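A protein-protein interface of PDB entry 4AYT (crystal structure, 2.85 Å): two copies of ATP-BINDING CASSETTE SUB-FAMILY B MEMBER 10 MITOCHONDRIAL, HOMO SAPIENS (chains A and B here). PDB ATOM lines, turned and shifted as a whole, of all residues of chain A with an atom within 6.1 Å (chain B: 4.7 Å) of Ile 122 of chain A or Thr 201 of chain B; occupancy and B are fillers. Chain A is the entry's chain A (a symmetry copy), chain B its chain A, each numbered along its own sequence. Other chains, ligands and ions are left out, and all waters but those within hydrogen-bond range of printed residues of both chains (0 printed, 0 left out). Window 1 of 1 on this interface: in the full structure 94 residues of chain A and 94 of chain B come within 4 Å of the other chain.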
ATOM      1  N   ARG A 117      12.409  -1.227  29.575  1.00  0.00           N
ATOM      2  CA  ARG A 117      13.268  -0.049  29.444  1.00  0.00           C
ATOM      3  C   ARG A 117      14.684  -0.476  29.041  1.00  0.00           C
ATOM      4  O   ARG A 117      15.148  -1.547  29.448  1.00  0.00           O
ATOM      5  CB  ARG A 117      13.281   0.779  30.743  1.00  0.00           C
ATOM      6  CG  ARG A 117      12.773   2.212  30.584  1.00  0.00           C
ATOM      7  N   THR A 118      15.342   0.348  28.198  1.00  0.00           N
ATOM      8  CA  THR A 118      16.692   0.110  27.660  1.00  0.00           C
ATOM      9  C   THR A 118      17.716   0.087  28.808  1.00  0.00           C
ATOM     10  O   THR A 118      18.605  -0.767  28.805  1.00  0.00           O
ATOM     11  CB  THR A 118      17.033   1.161  26.569  1.00  0.00           C
ATOM     12  OG1 THR A 118      15.988   1.185  25.589  1.00  0.00           O
ATOM     13  CG2 THR A 118      18.376   0.900  25.881  1.00  0.00           C
ATOM     14  N   GLY A 119      17.549   0.992  29.784  1.00  0.00           N
ATOM     15  CA  GLY A 119      18.390   1.087  30.972  1.00  0.00           C
ATOM     16  C   GLY A 119      18.465  -0.223  31.731  1.00  0.00           C
ATOM     17  O   GLY A 119      19.559  -0.646  32.117  1.00  0.00           O
ATOM     18  N   GLU A 120      17.300  -0.905  31.892  1.00  0.00           N
ATOM     19  CA  GLU A 120      17.202  -2.207  32.552  1.00  0.00           C
ATOM     20  C   GLU A 120      17.915  -3.292  31.752  1.00  0.00           C
ATOM     21  O   GLU A 120      18.532  -4.174  32.348  1.00  0.00           O
ATOM     22  CB  GLU A 120      15.738  -2.612  32.820  1.00  0.00           C
ATOM     23  CG  GLU A 120      15.571  -3.704  33.879  1.00  0.00           C
ATOM     24  CD  GLU A 120      16.525  -3.733  35.073  1.00  0.00           C
ATOM     25  OE1 GLU A 120      16.720  -2.677  35.725  1.00  0.00           O
ATOM     26  OE2 GLU A 120      17.071  -4.825  35.359  1.00  0.00           O
ATOM     27  N   LEU A 121      17.857  -3.217  30.410  1.00  0.00           N
ATOM     28  CA  LEU A 121      18.518  -4.186  29.532  1.00  0.00           C
ATOM     29  C   LEU A 121      20.016  -3.951  29.526  1.00  0.00           C
ATOM     30  O   LEU A 121      20.760  -4.920  29.506  1.00  0.00           O
ATOM     31  CB  LEU A 121      17.948  -4.143  28.098  1.00  0.00           C
ATOM     32  CG  LEU A 121      16.492  -4.623  27.916  1.00  0.00           C
ATOM     33  CD1 LEU A 121      15.973  -4.280  26.536  1.00  0.00           C
ATOM     34  CD2 LEU A 121      16.349  -6.110  28.176  1.00  0.00           C
ATOM     35  N   ILE A 122      20.458  -2.681  29.597  1.00  0.00           N
ATOM     36  CA  ILE A 122      21.883  -2.320  29.632  1.00  0.00           C
ATOM     37  C   ILE A 122      22.467  -2.680  31.015  1.00  0.00           C
ATOM     38  O   ILE A 122      23.555  -3.269  31.066  1.00  0.00           O
ATOM     39  CB  ILE A 122      22.116  -0.840  29.243  1.00  0.00           C
ATOM     40  CG1 ILE A 122      21.717  -0.575  27.776  1.00  0.00           C
ATOM     41  CG2 ILE A 122      23.544  -0.390  29.540  1.00  0.00           C
ATOM     42  CD1 ILE A 122      22.249  -1.620  26.755  1.00  0.00           C
ATOM     43  N   ASN A 123      21.725  -2.387  32.121  1.00  0.00           N
ATOM     44  CA  ASN A 123      22.137  -2.770  33.474  1.00  0.00           C
ATOM     45  C   ASN A 123      22.268  -4.297  33.582  1.00  0.00           C
ATOM     46  O   ASN A 123      23.211  -4.765  34.217  1.00  0.00           O
ATOM     47  CB  ASN A 123      21.186  -2.219  34.540  1.00  0.00           C
ATOM     48  CG  ASN A 123      21.379  -0.734  34.788  1.00  0.00           C
ATOM     49  OD1 ASN A 123      22.505  -0.238  34.951  1.00  0.00           O
ATOM     50  ND2 ASN A 123      20.285   0.018  34.817  1.00  0.00           N
ATOM     51  N   ARG A 124      21.391  -5.067  32.896  1.00  0.00           N
ATOM     52  CA  ARG A 124      21.474  -6.535  32.874  1.00  0.00           C
ATOM     53  C   ARG A 124      22.662  -7.033  32.025  1.00  0.00           C
ATOM     54  O   ARG A 124      23.213  -8.093  32.318  1.00  0.00           O
ATOM     55  CB  ARG A 124      20.171  -7.170  32.376  1.00  0.00           C
ATOM     56  CG  ARG A 124      19.071  -7.153  33.424  1.00  0.00           C
ATOM     57  CD  ARG A 124      17.881  -7.995  33.039  1.00  0.00           C
ATOM     58  NE  ARG A 124      16.659  -7.484  33.660  1.00  0.00           N
ATOM     59  CZ  ARG A 124      15.552  -8.199  33.846  1.00  0.00           C
ATOM     60  NH1 ARG A 124      15.501  -9.471  33.461  1.00  0.00           N
ATOM     61  NH2 ARG A 124      14.493  -7.653  34.431  1.00  0.00           N
ATOM     62  N   LEU A 125      23.058  -6.264  30.993  1.00  0.00           N
ATOM     63  CA  LEU A 125      24.151  -6.612  30.085  1.00  0.00           C
ATOM     64  C   LEU A 125      25.496  -6.118  30.634  1.00  0.00           C
ATOM     65  O   LEU A 125      26.533  -6.654  30.233  1.00  0.00           O
ATOM     66  CB  LEU A 125      23.862  -6.036  28.674  1.00  0.00           C
ATOM     67  CG  LEU A 125      24.840  -6.326  27.532  1.00  0.00           C
ATOM     68  CD1 LEU A 125      24.754  -7.767  27.058  1.00  0.00           C
ATOM     69  CD2 LEU A 125      24.605  -5.385  26.390  1.00  0.00           C
ATOM     70  N   SER A 126      25.484  -5.126  31.563  1.00  0.00           N
ATOM     71  CA  SER A 126      26.702  -4.580  32.170  1.00  0.00           C
ATOM     72  C   SER A 126      26.943  -5.139  33.571  1.00  0.00           C
ATOM     73  O   SER A 126      27.880  -5.913  33.771  1.00  0.00           O
ATOM     74  CB  SER A 126      26.645  -3.061  32.232  1.00  0.00           C
ATOM     75  OG  SER A 126      26.511  -2.503  30.937  1.00  0.00           O
ATOM     76  N   SER A 127      26.086  -4.775  34.529  1.00  0.00           N
ATOM     77  CA  SER A 127      26.256  -5.164  35.923  1.00  0.00           C
ATOM     78  C   SER A 127      25.952  -6.642  36.228  1.00  0.00           C
ATOM     79  O   SER A 127      26.744  -7.259  36.946  1.00  0.00           O
ATOM     80  CB  SER A 127      25.418  -4.276  36.832  1.00  0.00           C
ATOM     81  OG  SER A 127      25.889  -4.442  38.157  1.00  0.00           O
ATOM     82  N   LEU B 197      35.079  -1.377  26.397  1.00  0.00           N
ATOM     83  CA  LEU B 197      33.838  -1.920  26.932  1.00  0.00           C
ATOM     84  C   LEU B 197      32.739  -0.862  26.888  1.00  0.00           C
ATOM     85  O   LEU B 197      31.578  -1.213  26.672  1.00  0.00           O
ATOM     86  CB  LEU B 197      34.035  -2.450  28.353  1.00  0.00           C
ATOM     87  CG  LEU B 197      32.790  -3.008  29.024  1.00  0.00           C
ATOM     88  CD1 LEU B 197      32.248  -4.237  28.273  1.00  0.00           C
ATOM     89  CD2 LEU B 197      33.039  -3.283  30.483  1.00  0.00           C
ATOM     90  N   ALA B 198      33.093   0.425  27.087  1.00  0.00           N
ATOM     91  CA  ALA B 198      32.120   1.511  27.011  1.00  0.00           C
ATOM     92  C   ALA B 198      31.575   1.602  25.582  1.00  0.00           C
ATOM     93  O   ALA B 198      30.361   1.664  25.402  1.00  0.00           O
ATOM     94  CB  ALA B 198      32.750   2.831  27.439  1.00  0.00           C
ATOM     95  N   GLN B 199      32.474   1.523  24.569  1.00  0.00           N
ATOM     96  CA  GLN B 199      32.136   1.554  23.148  1.00  0.00           C
ATOM     97  C   GLN B 199      31.189   0.413  22.815  1.00  0.00           C
ATOM     98  O   GLN B 199      30.145   0.670  22.220  1.00  0.00           O
ATOM     99  CB  GLN B 199      33.397   1.470  22.274  1.00  0.00           C
ATOM    100  CG  GLN B 199      34.224   2.743  22.237  1.00  0.00           C
ATOM    101  CD  GLN B 199      35.234   2.702  21.116  1.00  0.00           C
ATOM    102  OE1 GLN B 199      36.192   1.917  21.131  1.00  0.00           O
ATOM    103  NE2 GLN B 199      35.041   3.552  20.118  1.00  0.00           N
ATOM    104  N   ALA B 200      31.516  -0.828  23.260  1.00  0.00           N
ATOM    105  CA  ALA B 200      30.705  -2.031  23.052  1.00  0.00           C
ATOM    106  C   ALA B 200      29.315  -1.880  23.637  1.00  0.00           C
ATOM    107  O   ALA B 200      28.356  -2.326  23.006  1.00  0.00           O
ATOM    108  CB  ALA B 200      31.380  -3.235  23.672  1.00  0.00           C
ATOM    109  N   THR B 201      29.201  -1.232  24.823  1.00  0.00           N
ATOM    110  CA  THR B 201      27.952  -0.990  25.546  1.00  0.00           C
ATOM    111  C   THR B 201      27.152   0.096  24.837  1.00  0.00           C
ATOM    112  O   THR B 201      25.931  -0.030  24.746  1.00  0.00           O
ATOM    113  CB  THR B 201      28.261  -0.653  27.001  1.00  0.00           C
ATOM    114  OG1 THR B 201      28.923  -1.780  27.580  1.00  0.00           O
ATOM    115  CG2 THR B 201      27.019  -0.326  27.820  1.00  0.00           C
ATOM    116  N   GLN B 202      27.832   1.130  24.300  1.00  0.00           N
ATOM    117  CA  GLN B 202      27.176   2.219  23.569  1.00  0.00           C
ATOM    118  C   GLN B 202      26.568   1.685  22.291  1.00  0.00           C
ATOM    119  O   GLN B 202      25.413   2.002  22.000  1.00  0.00           O
ATOM    120  CB  GLN B 202      28.132   3.390  23.275  1.00  0.00           C
ATOM    121  CG  GLN B 202      27.400   4.706  22.975  1.00  0.00           C
ATOM    122  CD  GLN B 202      26.327   5.041  23.998  1.00  0.00           C
ATOM    123  OE1 GLN B 202      26.579   5.122  25.211  1.00  0.00           O
ATOM    124  NE2 GLN B 202      25.099   5.218  23.527  1.00  0.00           N
ATOM    125  N   LEU B 203      27.321   0.822  21.573  1.00  0.00           N
ATOM    126  CA  LEU B 203      26.846   0.135  20.375  1.00  0.00           C
ATOM    127  C   LEU B 203      25.573  -0.627  20.721  1.00  0.00           C
ATOM    128  O   LEU B 203      24.536  -0.380  20.111  1.00  0.00           O
ATOM    129  CB  LEU B 203      27.908  -0.819  19.810  1.00  0.00           C
ATOM    130  CG  LEU B 203      27.393  -1.738  18.706  1.00  0.00           C
ATOM    131  CD1 LEU B 203      27.401  -1.061  17.394  1.00  0.00           C
ATOM    132  CD2 LEU B 203      28.195  -3.005  18.618  1.00  0.00           C
ATOM    133  N   ALA B 204      25.655  -1.499  21.749  1.00  0.00           N
ATOM    134  CA  ALA B 204      24.564  -2.302  22.273  1.00  0.00           C
ATOM    135  C   ALA B 204      23.353  -1.435  22.639  1.00  0.00           C
ATOM    136  O   ALA B 204      22.269  -1.666  22.096  1.00  0.00           O
ATOM    137  CB  ALA B 204      25.034  -3.084  23.482  1.00  0.00           C
ATOM    138  N   GLU B 205      23.556  -0.415  23.502  1.00  0.00           N
ATOM    139  CA  GLU B 205      22.524   0.511  23.994  1.00  0.00           C
ATOM    140  C   GLU B 205      21.768   1.186  22.843  1.00  0.00           C
ATOM    141  O   GLU B 205      20.531   1.202  22.854  1.00  0.00           O
ATOM    142  CB  GLU B 205      23.174   1.561  24.921  1.00  0.00           C
ATOM    143  CG  GLU B 205      22.268   2.651  25.465  1.00  0.00           C
ATOM    144  CD  GLU B 205      22.923   3.462  26.563  1.00  0.00           C
ATOM    145  OE1 GLU B 205      24.048   3.973  26.345  1.00  0.00           O
ATOM    146  OE2 GLU B 205      22.321   3.564  27.658  1.00  0.00           O
ATOM    147  N   ILE B 208      19.671  -1.469  20.720  1.00  0.00           N
ATOM    148  CA  ILE B 208      18.492  -1.872  21.506  1.00  0.00           C
ATOM    149  C   ILE B 208      17.462  -0.727  21.520  1.00  0.00           C
ATOM    150  O   ILE B 208      16.263  -0.953  21.329  1.00  0.00           O
ATOM    151  CB  ILE B 208      18.904  -2.287  22.943  1.00  0.00           C
ATOM    152  CG1 ILE B 208      19.654  -3.653  22.917  1.00  0.00           C
ATOM    153  CG2 ILE B 208      17.680  -2.326  23.865  1.00  0.00           C
ATOM    154  CD1 ILE B 208      20.680  -3.854  23.980  1.00  0.00           C
ATOM    155  N   TYR B 227      28.779  -6.710  17.728  1.00  0.00           N
ATOM    156  CA  TYR B 227      28.923  -6.637  19.189  1.00  0.00           C
ATOM    157  C   TYR B 227      29.829  -7.762  19.700  1.00  0.00           C
ATOM    158  O   TYR B 227      30.755  -7.485  20.452  1.00  0.00           O
ATOM    159  CB  TYR B 227      27.555  -6.688  19.887  1.00  0.00           C
ATOM    160  CG  TYR B 227      27.649  -6.659  21.397  1.00  0.00           C
ATOM    161  CD1 TYR B 227      27.826  -5.460  22.080  1.00  0.00           C
ATOM    162  CD2 TYR B 227      27.539  -7.826  22.146  1.00  0.00           C
ATOM    163  CE1 TYR B 227      27.910  -5.424  23.472  1.00  0.00           C
ATOM    164  CE2 TYR B 227      27.635  -7.806  23.536  1.00  0.00           C
ATOM    165  CZ  TYR B 227      27.806  -6.598  24.199  1.00  0.00           C
ATOM    166  OH  TYR B 227      27.922  -6.553  25.569  1.00  0.00           O
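Thr 118 of chain A touches Glu 205 of chain B. CG2 of Ile 208 of chain B touches CG2 of Thr 118 of chain A (3.9 Å). CD1 of Leu 121 of chain A touches CG2 of Ile 208 of chain B, at 3.7 Å. Thr 201 of chain B touches Ile 122 of chain A. Ile 122 of chain A touches Glu 205 of chain B. Ile 122 of chain A touches Ile 208 of chain B (CD1 to CD1, 3.9 Å). Leu 125 of chain A touches Ala 204 of chain B (CD2 to CB, 3.7 Å). Leu 125 of chain A touches Tyr 227 of chain B (CD2 to OH, 3.6 Å). OG of Ser 126 of chain A touches CG2 of Thr 201 of chain B, 3.8 Å away.
Ile 122 of chain A touches just these residues of chain B: Thr 201 (3.9 Å), Glu 205 (3.5 Å) and Ile 208 (3.9 Å). Printed residues of chain A within 4 Å of Tyr 227 of chain B: Leu 125 (3.6 Å). Printed residues of chain B within 4 Å of Ser 126 of chain A: Thr 201. Of the printed residues of chain B, Thr 118 of chain A touches Glu 205 (3.7 Å) and Ile 208 (3.9 Å). The nearest residue of chain B that does not touch Ile 122 of chain A is Ala 204 of chain B (4.3 Å). The nearest printed residue of chain A that does not touch Ala 204 of chain B is Ile 122 of chain A (4.3 Å).
No position is printed for both chains. Of the 9 pairs that touch across the chains among the printed residues, none has its exchanged pair printed and touching as well.
O of Leu 197 of chain B lies within hydrogen-bond range of OG1 of Thr 201 of chain B, at 2.9 Å. The side-chain amide oxygen (OE1) of Gln 202 of chain B lies close to the side-chain carboxylate (OE1) of Glu 205 of chain B. The backbone carbonyl oxygen (O) of Ile 122 of chain A lies within hydrogen-bond range of the side-chain hydroxyl (OG) of Ser 126 of chain A.
Of the 11 printed residues of chain A, 5 touch a printed residue of chain B. Of the 11 printed residues of chain B, 5 touch a printed residue of chain A. Printed residues of chain B that touch a printed residue of chain A: Thr 201, Ala 204, Glu 205, Ile 208 and Tyr 227. Hydrophobic or aromatic side chains of chain B that line the printed part of chain A: Ala 204, Ile 208 and Tyr 227. Among the printed residues, 9 pairs touch across the chains. Among the printed residues, no Asp or Glu carboxylate lies within 4 Å of a Lys or Arg side-chain nitrogen of the other chain.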
